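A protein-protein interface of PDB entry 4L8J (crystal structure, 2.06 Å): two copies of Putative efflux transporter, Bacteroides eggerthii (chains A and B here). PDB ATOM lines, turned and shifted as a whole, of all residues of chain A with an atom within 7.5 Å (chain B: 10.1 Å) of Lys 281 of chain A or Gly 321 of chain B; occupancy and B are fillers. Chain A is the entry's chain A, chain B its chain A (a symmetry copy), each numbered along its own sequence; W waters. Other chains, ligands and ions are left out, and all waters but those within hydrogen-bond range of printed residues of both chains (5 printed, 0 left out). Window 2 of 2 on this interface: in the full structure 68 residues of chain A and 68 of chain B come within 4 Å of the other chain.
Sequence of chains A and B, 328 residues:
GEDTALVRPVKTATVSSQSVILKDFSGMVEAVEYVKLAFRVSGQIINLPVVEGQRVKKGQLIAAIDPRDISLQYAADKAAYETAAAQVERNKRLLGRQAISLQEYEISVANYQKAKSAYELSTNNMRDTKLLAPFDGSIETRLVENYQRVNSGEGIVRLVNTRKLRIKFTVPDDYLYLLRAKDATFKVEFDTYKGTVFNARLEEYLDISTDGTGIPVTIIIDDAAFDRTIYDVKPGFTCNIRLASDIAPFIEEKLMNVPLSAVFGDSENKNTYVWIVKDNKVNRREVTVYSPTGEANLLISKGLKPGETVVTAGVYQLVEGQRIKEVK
Among the printed residues, merely in contact across the chains: Trp 275 of chain A with Val 310 of chain B, Lys 281 of chain A with Gln 322 of chain B, Ile 276 of chain A with Thr 309 of chain B, Thr 4 of chain A with Glu 320 of chain B, Asn 280 of chain A with Arg 323 of chain B, Trp 275 of chain A with Leu 318 of chain B, Lys 281 of chain A with Gly 321 of chain B, Val 277 of chain A with Glu 326 of chain B, Thr 4 of chain A with Gln 322 of chain B, Val 277 of chain A with Val 311 of chain B, Val 282 of chain A with Val 311 of chain B, Trp 275 of chain A with Glu 320 of chain B, Val 282 of chain A with Val 319 of chain B, Val 277 of chain A with Ile 324 of chain B, Val 282 of chain A with Ile 324 of chain B, Trp 275 of chain A with Thr 309 of chain B, Ile 276 of chain A with Val 310 of chain B, Trp 275 of chain A with Val 319 of chain B, Thr 4 of chain A with Gly 321 of chain B and Val 282 of chain A with Glu 320 of chain B.
Of the 13 printed residues of chain B, 11 touch a printed residue of chain A. Hydrophobic or aromatic side chains of chain B within 4 Å of the printed part of chain A: Val 310, Val 311, Leu 318 and Ile 324. Among the printed residues, 29 pairs touch across the chains. Among the printed residues, no Asp or Glu carboxylate lies within 4 Å of a Lys or Arg side-chain nitrogen of the other chain.
Of the printed residues of chain A, Gly 321 of chain B touches Thr 4 (3.8 Å), Lys 281 (3.5 Å) and Val 282 (2.7 Å). Val 277 of chain A touches just these residues of chain B: Thr 309, Val 311, Ile 324 and Glu 326. Asn 280 of chain A touches just these residues of chain B: Arg 323 (3.4 Å) and Ile 324 (2.8 Å). Of the printed residues of chain B, Val 282 of chain A touches Val 311, Val 319, Glu 320, Gly 321, Gln 322 and Ile 324. Of the printed residues of chain A, Val 310 of chain B touches Trp 275 (3.2 Å) and Ile 276 (3.8 Å). Of the printed residues of chain A, Val 319 of chain B touches Trp 275 (3.8 Å) and Val 282 (3.7 Å). Printed residues of chain A within 4 Å of Thr 309 of chain B: Trp 275 (3.8 Å), Ile 276 (3.3 Å) and Val 277 (2.7 Å). Of the printed residues of chain A, Arg 323 of chain B touches Thr 4 and Asn 280. Printed residues of chain B within 4 Å of Trp 275 of chain A: Thr 309, Val 310, Val 311, Leu 318, Val 319 and Glu 320. Ala 5 of chain A touches none of the printed residues of chain B. Lys 278 of chain A touches none of the printed residues of chain B. The nearest residue of chain B that does not touch Lys 281 of chain A is Ile 324 of chain B (4.2 Å). The nearest printed residue of chain A that does not touch Glu 320 of chain B is Lys 281 of chain A (7.0 Å).
The side-chain carboxylate (OD1) of Asp 3 of chain A sits at hydrogen-bond distance from the backbone NH (N) of Ala 5 of chain A (3.2 Å). N of Ile 276 of chain A is in hydrogen-bond range of O of Asn 283 of chain A. The backbone NH of Val 319 of chain B is in hydrogen-bond range of the side-chain amide oxygen of Gln 322 of chain B (3.1 Å).
No position is printed for both chains. Of the 29 pairs that touch across the chains among the printed residues, none has its exchanged pair printed and touching as well.
Water W1 bridges OD1 of Asn 280 of chain A (2.6 Å) and N of Glu 326 of chain B (2.8 Å). Water W2 lies within hydrogen-bond range of O of Val 311 of chain B (2.7 Å) and N of Trp 275 of chain A (2.8 Å). Water W3 bridges the backbone carbonyl oxygen of Arg 284 of chain A (2.7 Å) and the side-chain carboxylate of Glu 320 of chain B (2.8 Å). Water W4 lies within hydrogen-bond range of the backbone carbonyl oxygen (O) of Val 277 of chain A (2.8 Å) and the backbone NH (N) of Thr 309 of chain B (2.8 Å). Water W5 bridges the guanidinium group (NH1) of Arg 323 of chain B (2.8 Å) and the backbone carbonyl oxygen (O) of Asn 280 of chain A (2.9 Å).
NE2 of Gln 322 of chain B sits at hydrogen-bond distance from O of Asp 3 of chain A (3.3 Å). O of Thr 4 of chain A sits at hydrogen-bond distance from N of Arg 323 of chain B (2.9 Å). The backbone carbonyl oxygen (O) of Trp 275 of chain A sits at hydrogen-bond distance from the backbone NH (N) of Val 311 of chain B. The backbone NH (N) of Val 277 of chain A sits at hydrogen-bond distance from the backbone carbonyl oxygen (O) of Thr 309 of chain B (2.7 Å). The backbone carbonyl oxygen (O) of Asn 280 of chain A sits at hydrogen-bond distance from the backbone NH (N) of Ile 324 of chain B, 2.8 Å away. N of Gly 321 of chain B is in hydrogen-bond range of O of Val 282 of chain A (2.7 Å). The backbone NH (N) of Val 282 of chain A lies within hydrogen-bond range of the backbone carbonyl oxygen (O) of Gln 322 of chain B (3.0 Å). ND2 of Asn 283 of chain A lies within hydrogen-bond range of OE2 of Glu 320 of chain B, at 2.6 Å. N of Arg 284 of chain A lies within hydrogen-bond range of OE1 of Glu 320 of chain B (2.8 Å).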
ATOM      1  N   ASP A   3     -24.741  14.243  17.495  1.00  0.00           N
ATOM      2  CA  ASP A   3     -25.951  13.534  17.902  1.00  0.00           C
ATOM      3  C   ASP A   3     -25.699  12.005  17.899  1.00  0.00           C
ATOM      4  O   ASP A   3     -24.540  11.584  17.941  1.00  0.00           O
ATOM      5  CB  ASP A   3     -27.122  13.925  16.971  1.00  0.00           C
ATOM      6  CG  ASP A   3     -27.100  13.345  15.558  1.00  0.00           C
ATOM      7  OD1 ASP A   3     -25.993  13.200  14.986  1.00  0.00           O
ATOM      8  OD2 ASP A   3     -28.193  13.033  15.029  1.00  0.00           O
ATOM      9  N   THR A   4     -26.775  11.182  17.856  1.00  0.00           N
ATOM     10  CA  THR A   4     -26.668   9.721  17.804  1.00  0.00           C
ATOM     11  C   THR A   4     -26.236   9.275  16.370  1.00  0.00           C
ATOM     12  O   THR A   4     -25.626   8.215  16.211  1.00  0.00           O
ATOM     13  CB  THR A   4     -27.990   9.042  18.251  1.00  0.00           C
ATOM     14  OG1 THR A   4     -29.067   9.494  17.425  1.00  0.00           O
ATOM     15  CG2 THR A   4     -28.317   9.266  19.747  1.00  0.00           C
ATOM     16  N   ALA A   5     -26.558  10.100  15.339  1.00  0.00           N
ATOM     17  CA  ALA A   5     -26.209   9.831  13.937  1.00  0.00           C
ATOM     18  C   ALA A   5     -24.696  10.030  13.681  1.00  0.00           C
ATOM     19  O   ALA A   5     -24.174   9.476  12.703  1.00  0.00           O
ATOM     20  CB  ALA A   5     -27.025  10.716  13.009  1.00  0.00           C
ATOM     21  N   TRP A 275     -20.740   0.895  28.501  1.00  0.00           N
ATOM     22  CA  TRP A 275     -21.483   1.054  27.249  1.00  0.00           C
ATOM     23  C   TRP A 275     -21.551  -0.312  26.614  1.00  0.00           C
ATOM     24  O   TRP A 275     -20.501  -0.877  26.306  1.00  0.00           O
ATOM     25  CB  TRP A 275     -20.808   2.050  26.281  1.00  0.00           C
ATOM     26  CG  TRP A 275     -20.841   3.495  26.670  1.00  0.00           C
ATOM     27  CD1 TRP A 275     -19.767   4.295  26.944  1.00  0.00           C
ATOM     28  CD2 TRP A 275     -22.003   4.332  26.755  1.00  0.00           C
ATOM     29  NE1 TRP A 275     -20.188   5.581  27.198  1.00  0.00           N
ATOM     30  CE2 TRP A 275     -21.559   5.629  27.103  1.00  0.00           C
ATOM     31  CE3 TRP A 275     -23.380   4.120  26.533  1.00  0.00           C
ATOM     32  CZ2 TRP A 275     -22.446   6.710  27.256  1.00  0.00           C
ATOM     33  CZ3 TRP A 275     -24.253   5.185  26.684  1.00  0.00           C
ATOM     34  CH2 TRP A 275     -23.789   6.455  27.077  1.00  0.00           C
ATOM     35  N   ILE A 276     -22.752  -0.860  26.456  1.00  0.00           N
ATOM     36  CA  ILE A 276     -22.993  -2.116  25.760  1.00  0.00           C
ATOM     37  C   ILE A 276     -23.152  -1.797  24.260  1.00  0.00           C
ATOM     38  O   ILE A 276     -23.925  -0.910  23.903  1.00  0.00           O
ATOM     39  CB  ILE A 276     -24.244  -2.868  26.341  1.00  0.00           C
ATOM     40  CG1 ILE A 276     -23.940  -3.494  27.728  1.00  0.00           C
ATOM     41  CG2 ILE A 276     -24.793  -3.986  25.349  1.00  0.00           C
ATOM     42  CD1 ILE A 276     -23.000  -4.691  27.683  1.00  0.00           C
ATOM     43  N   VAL A 277     -22.445  -2.535  23.404  1.00  0.00           N
ATOM     44  CA  VAL A 277     -22.520  -2.395  21.955  1.00  0.00           C
ATOM     45  C   VAL A 277     -23.454  -3.473  21.407  1.00  0.00           C
ATOM     46  O   VAL A 277     -23.145  -4.657  21.494  1.00  0.00           O
ATOM     47  CB  VAL A 277     -21.128  -2.481  21.293  1.00  0.00           C
ATOM     48  CG1 VAL A 277     -21.232  -2.323  19.771  1.00  0.00           C
ATOM     49  CG2 VAL A 277     -20.187  -1.446  21.885  1.00  0.00           C
ATOM     50  N   LYS A 278     -24.593  -3.047  20.867  1.00  0.00           N
ATOM     51  CA  LYS A 278     -25.587  -3.892  20.210  1.00  0.00           C
ATOM     52  C   LYS A 278     -25.978  -3.214  18.901  1.00  0.00           C
ATOM     53  O   LYS A 278     -26.362  -2.038  18.917  1.00  0.00           O
ATOM     54  CB  LYS A 278     -26.825  -4.139  21.103  1.00  0.00           C
ATOM     55  CG  LYS A 278     -27.685  -5.315  20.621  1.00  0.00           C
ATOM     56  CD  LYS A 278     -27.153  -6.654  21.167  1.00  0.00           C
ATOM     57  CE  LYS A 278     -27.262  -7.816  20.205  1.00  0.00           C
ATOM     58  NZ  LYS A 278     -26.544  -9.013  20.723  1.00  0.00           N
ATOM     59  N   ASP A 279     -25.813  -3.944  17.784  1.00  0.00           N
ATOM     60  CA  ASP A 279     -26.096  -3.542  16.401  1.00  0.00           C
ATOM     61  C   ASP A 279     -25.418  -2.185  16.084  1.00  0.00           C
ATOM     62  O   ASP A 279     -26.083  -1.220  15.690  1.00  0.00           O
ATOM     63  CB  ASP A 279     -27.623  -3.494  16.137  1.00  0.00           C
ATOM     64  CG  ASP A 279     -28.348  -4.809  16.401  1.00  0.00           C
ATOM     65  OD1 ASP A 279     -27.876  -5.866  15.894  1.00  0.00           O
ATOM     66  OD2 ASP A 279     -29.404  -4.779  17.087  1.00  0.00           O
ATOM     67  N   ASN A 280     -24.099  -2.108  16.367  1.00  0.00           N
ATOM     68  CA  ASN A 280     -23.239  -0.939  16.129  1.00  0.00           C
ATOM     69  C   ASN A 280     -23.801   0.376  16.747  1.00  0.00           C
ATOM     70  O   ASN A 280     -23.546   1.468  16.222  1.00  0.00           O
ATOM     71  CB  ASN A 280     -22.968  -0.780  14.616  1.00  0.00           C
ATOM     72  CG  ASN A 280     -21.952  -1.771  14.086  1.00  0.00           C
ATOM     73  OD1 ASN A 280     -20.737  -1.666  14.332  1.00  0.00           O
ATOM     74  ND2 ASN A 280     -22.425  -2.743  13.320  1.00  0.00           N
ATOM     75  N   LYS A 281     -24.536   0.257  17.881  1.00  0.00           N
ATOM     76  CA  LYS A 281     -25.044   1.374  18.701  1.00  0.00           C
ATOM     77  C   LYS A 281     -24.716   1.101  20.181  1.00  0.00           C
ATOM     78  O   LYS A 281     -24.621  -0.061  20.589  1.00  0.00           O
ATOM     79  CB  LYS A 281     -26.553   1.609  18.552  1.00  0.00           C
ATOM     80  CG  LYS A 281     -27.060   2.026  17.168  1.00  0.00           C
ATOM     81  CD  LYS A 281     -28.565   1.717  17.025  1.00  0.00           C
ATOM     82  CE  LYS A 281     -29.472   2.573  17.907  1.00  0.00           C
ATOM     83  NZ  LYS A 281     -30.830   1.982  18.087  1.00  0.00           N
ATOM     84  N   VAL A 282     -24.559   2.156  20.974  1.00  0.00           N
ATOM     85  CA  VAL A 282     -24.256   1.988  22.395  1.00  0.00           C
ATOM     86  C   VAL A 282     -25.459   2.332  23.259  1.00  0.00           C
ATOM     87  O   VAL A 282     -26.258   3.188  22.900  1.00  0.00           O
ATOM     88  CB  VAL A 282     -23.000   2.748  22.873  1.00  0.00           C
ATOM     89  CG1 VAL A 282     -21.743   2.181  22.219  1.00  0.00           C
ATOM     90  CG2 VAL A 282     -23.124   4.259  22.654  1.00  0.00           C
ATOM     91  N   ASN A 283     -25.582   1.618  24.387  1.00  0.00           N
ATOM     92  CA  ASN A 283     -26.607   1.800  25.421  1.00  0.00           C
ATOM     93  C   ASN A 283     -25.959   1.598  26.772  1.00  0.00           C
ATOM     94  O   ASN A 283     -25.236   0.612  26.979  1.00  0.00           O
ATOM     95  CB  ASN A 283     -27.788   0.847  25.236  1.00  0.00           C
ATOM     96  CG  ASN A 283     -28.575   1.132  23.977  1.00  0.00           C
ATOM     97  OD1 ASN A 283     -28.364   0.510  22.934  1.00  0.00           O
ATOM     98  ND2 ASN A 283     -29.459   2.115  24.036  1.00  0.00           N
ATOM     99  N   ARG A 284     -26.216   2.538  27.688  1.00  0.00           N
ATOM    100  CA  ARG A 284     -25.630   2.497  29.022  1.00  0.00           C
ATOM    101  C   ARG A 284     -26.202   1.329  29.847  1.00  0.00           C
ATOM    102  O   ARG A 284     -27.395   1.040  29.792  1.00  0.00           O
ATOM    103  CB  ARG A 284     -25.816   3.823  29.751  1.00  0.00           C
ATOM    104  CG  ARG A 284     -24.752   4.058  30.829  1.00  0.00           C
ATOM    105  CD  ARG A 284     -24.972   5.360  31.575  1.00  0.00           C
ATOM    106  NE  ARG A 284     -26.307   5.420  32.188  1.00  0.00           N
ATOM    107  CZ  ARG A 284     -26.654   6.286  33.133  1.00  0.00           C
ATOM    108  NH1 ARG A 284     -25.767   7.154  33.605  1.00  0.00           N
ATOM    109  NH2 ARG A 284     -27.883   6.274  33.633  1.00  0.00           N
ATOM    110  N   THR B 309     -20.741  -7.207  24.336  1.00  0.00           N
ATOM    111  CA  THR B 309     -19.667  -6.318  23.903  1.00  0.00           C
ATOM    112  C   THR B 309     -19.717  -4.980  24.653  1.00  0.00           C
ATOM    113  O   THR B 309     -20.742  -4.303  24.639  1.00  0.00           O
ATOM    114  CB  THR B 309     -19.754  -6.121  22.379  1.00  0.00           C
ATOM    115  OG1 THR B 309     -19.763  -7.406  21.774  1.00  0.00           O
ATOM    116  CG2 THR B 309     -18.601  -5.301  21.835  1.00  0.00           C
ATOM    117  N   VAL B 310     -18.588  -4.574  25.252  1.00  0.00           N
ATOM    118  CA  VAL B 310     -18.496  -3.282  25.953  1.00  0.00           C
ATOM    119  C   VAL B 310     -17.484  -2.357  25.240  1.00  0.00           C
ATOM    120  O   VAL B 310     -16.539  -2.851  24.648  1.00  0.00           O
ATOM    121  CB  VAL B 310     -18.153  -3.405  27.468  1.00  0.00           C
ATOM    122  CG1 VAL B 310     -19.270  -4.103  28.253  1.00  0.00           C
ATOM    123  CG2 VAL B 310     -16.810  -4.118  27.699  1.00  0.00           C
ATOM    124  N   VAL B 311     -17.658  -1.028  25.343  1.00  0.00           N
ATOM    125  CA  VAL B 311     -16.705  -0.035  24.821  1.00  0.00           C
ATOM    126  C   VAL B 311     -15.526   0.044  25.827  1.00  0.00           C
ATOM    127  O   VAL B 311     -15.783   0.141  27.017  1.00  0.00           O
ATOM    128  CB  VAL B 311     -17.395   1.350  24.643  1.00  0.00           C
ATOM    129  CG1 VAL B 311     -16.373   2.470  24.432  1.00  0.00           C
ATOM    130  CG2 VAL B 311     -18.417   1.321  23.502  1.00  0.00           C
ATOM    131  N   GLN B 317     -17.000  10.277  24.858  1.00  0.00           N
ATOM    132  CA  GLN B 317     -17.533  10.990  23.700  1.00  0.00           C
ATOM    133  C   GLN B 317     -18.796  10.302  23.156  1.00  0.00           C
ATOM    134  O   GLN B 317     -19.054  10.334  21.957  1.00  0.00           O
ATOM    135  CB  GLN B 317     -16.441  11.059  22.629  1.00  0.00           C
ATOM    136  CG  GLN B 317     -15.189  11.807  23.082  1.00  0.00           C
ATOM    137  CD  GLN B 317     -13.977  11.240  22.402  1.00  0.00           C
ATOM    138  OE1 GLN B 317     -13.488  10.153  22.744  1.00  0.00           O
ATOM    139  NE2 GLN B 317     -13.486  11.949  21.398  1.00  0.00           N
ATOM    140  N   LEU B 318     -19.583   9.687  24.034  1.00  0.00           N
ATOM    141  CA  LEU B 318     -20.772   8.932  23.626  1.00  0.00           C
ATOM    142  C   LEU B 318     -22.016   9.331  24.386  1.00  0.00           C
ATOM    143  O   LEU B 318     -21.940   9.715  25.552  1.00  0.00           O
ATOM    144  CB  LEU B 318     -20.530   7.420  23.844  1.00  0.00           C
ATOM    145  CG  LEU B 318     -19.486   6.774  22.963  1.00  0.00           C
ATOM    146  CD1 LEU B 318     -19.181   5.370  23.444  1.00  0.00           C
ATOM    147  CD2 LEU B 318     -19.927   6.758  21.509  1.00  0.00           C
ATOM    148  N   VAL B 319     -23.169   9.185  23.727  1.00  0.00           N
ATOM    149  CA  VAL B 319     -24.496   9.418  24.313  1.00  0.00           C
ATOM    150  C   VAL B 319     -25.368   8.171  24.045  1.00  0.00           C
ATOM    151  O   VAL B 319     -25.068   7.390  23.148  1.00  0.00           O
ATOM    152  CB  VAL B 319     -25.201  10.732  23.840  1.00  0.00           C
ATOM    153  CG1 VAL B 319     -24.343  11.961  24.126  1.00  0.00           C
ATOM    154  CG2 VAL B 319     -25.591  10.670  22.365  1.00  0.00           C
ATOM    155  N   GLU B 320     -26.425   7.983  24.846  1.00  0.00           N
ATOM    156  CA  GLU B 320     -27.358   6.862  24.744  1.00  0.00           C
ATOM    157  C   GLU B 320     -27.879   6.699  23.309  1.00  0.00           C
ATOM    158  O   GLU B 320     -28.368   7.660  22.727  1.00  0.00           O
ATOM    159  CB  GLU B 320     -28.533   7.106  25.722  1.00  0.00           C
ATOM    160  CG  GLU B 320     -29.506   5.940  25.846  1.00  0.00           C
ATOM    161  CD  GLU B 320     -28.931   4.654  26.413  1.00  0.00           C
ATOM    162  OE1 GLU B 320     -27.899   4.717  27.116  1.00  0.00           O
ATOM    163  OE2 GLU B 320     -29.539   3.585  26.187  1.00  0.00           O
ATOM    164  N   GLY B 321     -27.723   5.509  22.747  1.00  0.00           N
ATOM    165  CA  GLY B 321     -28.197   5.187  21.403  1.00  0.00           C
ATOM    166  C   GLY B 321     -27.294   5.588  20.254  1.00  0.00           C
ATOM    167  O   GLY B 321     -27.620   5.305  19.096  1.00  0.00           O
ATOM    168  N   GLN B 322     -26.157   6.248  20.543  1.00  0.00           N
ATOM    169  CA  GLN B 322     -25.248   6.723  19.486  1.00  0.00           C
ATOM    170  C   GLN B 322     -24.658   5.569  18.659  1.00  0.00           C
ATOM    171  O   GLN B 322     -24.270   4.541  19.201  1.00  0.00           O
ATOM    172  CB  GLN B 322     -24.110   7.566  20.086  1.00  0.00           C
ATOM    173  CG  GLN B 322     -23.226   8.241  19.032  1.00  0.00           C
ATOM    174  CD  GLN B 322     -22.388   9.379  19.569  1.00  0.00           C
ATOM    175  OE1 GLN B 322     -22.356   9.666  20.758  1.00  0.00           O
ATOM    176  NE2 GLN B 322     -21.709  10.083  18.684  1.00  0.00           N
ATOM    177  N   ARG B 323     -24.594   5.764  17.345  1.00  0.00           N
ATOM    178  CA  ARG B 323     -23.950   4.839  16.425  1.00  0.00           C
ATOM    179  C   ARG B 323     -22.436   4.846  16.649  1.00  0.00           C
ATOM    180  O   ARG B 323     -21.849   5.909  16.909  1.00  0.00           O
ATOM    181  CB  ARG B 323     -24.213   5.237  14.967  1.00  0.00           C
ATOM    182  CG  ARG B 323     -25.644   5.256  14.486  1.00  0.00           C
ATOM    183  CD  ARG B 323     -25.591   5.717  13.031  1.00  0.00           C
ATOM    184  NE  ARG B 323     -26.857   5.564  12.313  1.00  0.00           N
ATOM    185  CZ  ARG B 323     -27.283   4.426  11.772  1.00  0.00           C
ATOM    186  NH1 ARG B 323     -26.565   3.312  11.894  1.00  0.00           N
ATOM    187  NH2 ARG B 323     -28.439   4.388  11.119  1.00  0.00           N
ATOM    188  N   ILE B 324     -21.791   3.687  16.454  1.00  0.00           N
ATOM    189  CA  ILE B 324     -20.346   3.611  16.600  1.00  0.00           C
ATOM    190  C   ILE B 324     -19.738   2.839  15.449  1.00  0.00           C
ATOM    191  O   ILE B 324     -20.441   2.141  14.711  1.00  0.00           O
ATOM    192  CB  ILE B 324     -19.937   2.971  17.985  1.00  0.00           C
ATOM    193  CG1 ILE B 324     -20.544   1.563  18.218  1.00  0.00           C
ATOM    194  CG2 ILE B 324     -20.226   3.890  19.170  1.00  0.00           C
ATOM    195  CD1 ILE B 324     -19.780   0.413  17.592  1.00  0.00           C
ATOM    196  N   LYS B 325     -18.401   2.868  15.368  1.00  0.00           N
ATOM    197  CA  LYS B 325     -17.660   2.022  14.461  1.00  0.00           C
ATOM    198  C   LYS B 325     -16.581   1.366  15.307  1.00  0.00           C
ATOM    199  O   LYS B 325     -15.810   2.062  15.978  1.00  0.00           O
ATOM    200  CB  LYS B 325     -17.102   2.769  13.221  1.00  0.00           C
ATOM    201  CG  LYS B 325     -16.361   1.813  12.299  1.00  0.00           C
ATOM    202  CD  LYS B 325     -15.571   2.505  11.216  1.00  0.00           C
ATOM    203  CE  LYS B 325     -14.743   1.493  10.510  1.00  0.00           C
ATOM    204  NZ  LYS B 325     -15.382   1.027   9.280  1.00  0.00           N
ATOM    205  N   GLU B 326     -16.571   0.036  15.336  1.00  0.00           N
ATOM    206  CA  GLU B 326     -15.571  -0.693  16.094  1.00  0.00           C
ATOM    207  C   GLU B 326     -14.244  -0.604  15.351  1.00  0.00           C
ATOM    208  O   GLU B 326     -14.195  -0.890  14.152  1.00  0.00           O
ATOM    209  CB  GLU B 326     -16.009  -2.153  16.318  1.00  0.00           C
ATOM    210  CG  GLU B 326     -17.244  -2.264  17.215  1.00  0.00           C
ATOM    211  CD  GLU B 326     -17.552  -3.637  17.805  1.00  0.00           C
ATOM    212  OE1 GLU B 326     -16.605  -4.349  18.215  1.00  0.00           O
ATOM    213  OE2 GLU B 326     -18.752  -3.975  17.911  1.00  0.00           O
HETATM  214  O   HOH W   1     -18.248  -1.560  13.740  1.00  0.00           O
HETATM  215  O   HOH W   2     -17.916   1.036  28.424  1.00  0.00           O
HETATM  216  O   HOH W   3     -29.594   2.058  28.546  1.00  0.00           O
HETATM  217  O   HOH W   4     -23.388  -6.737  23.398  1.00  0.00           O
HETATM  218  O   HOH W   5     -24.636   2.160  13.641  1.00  0.00           O
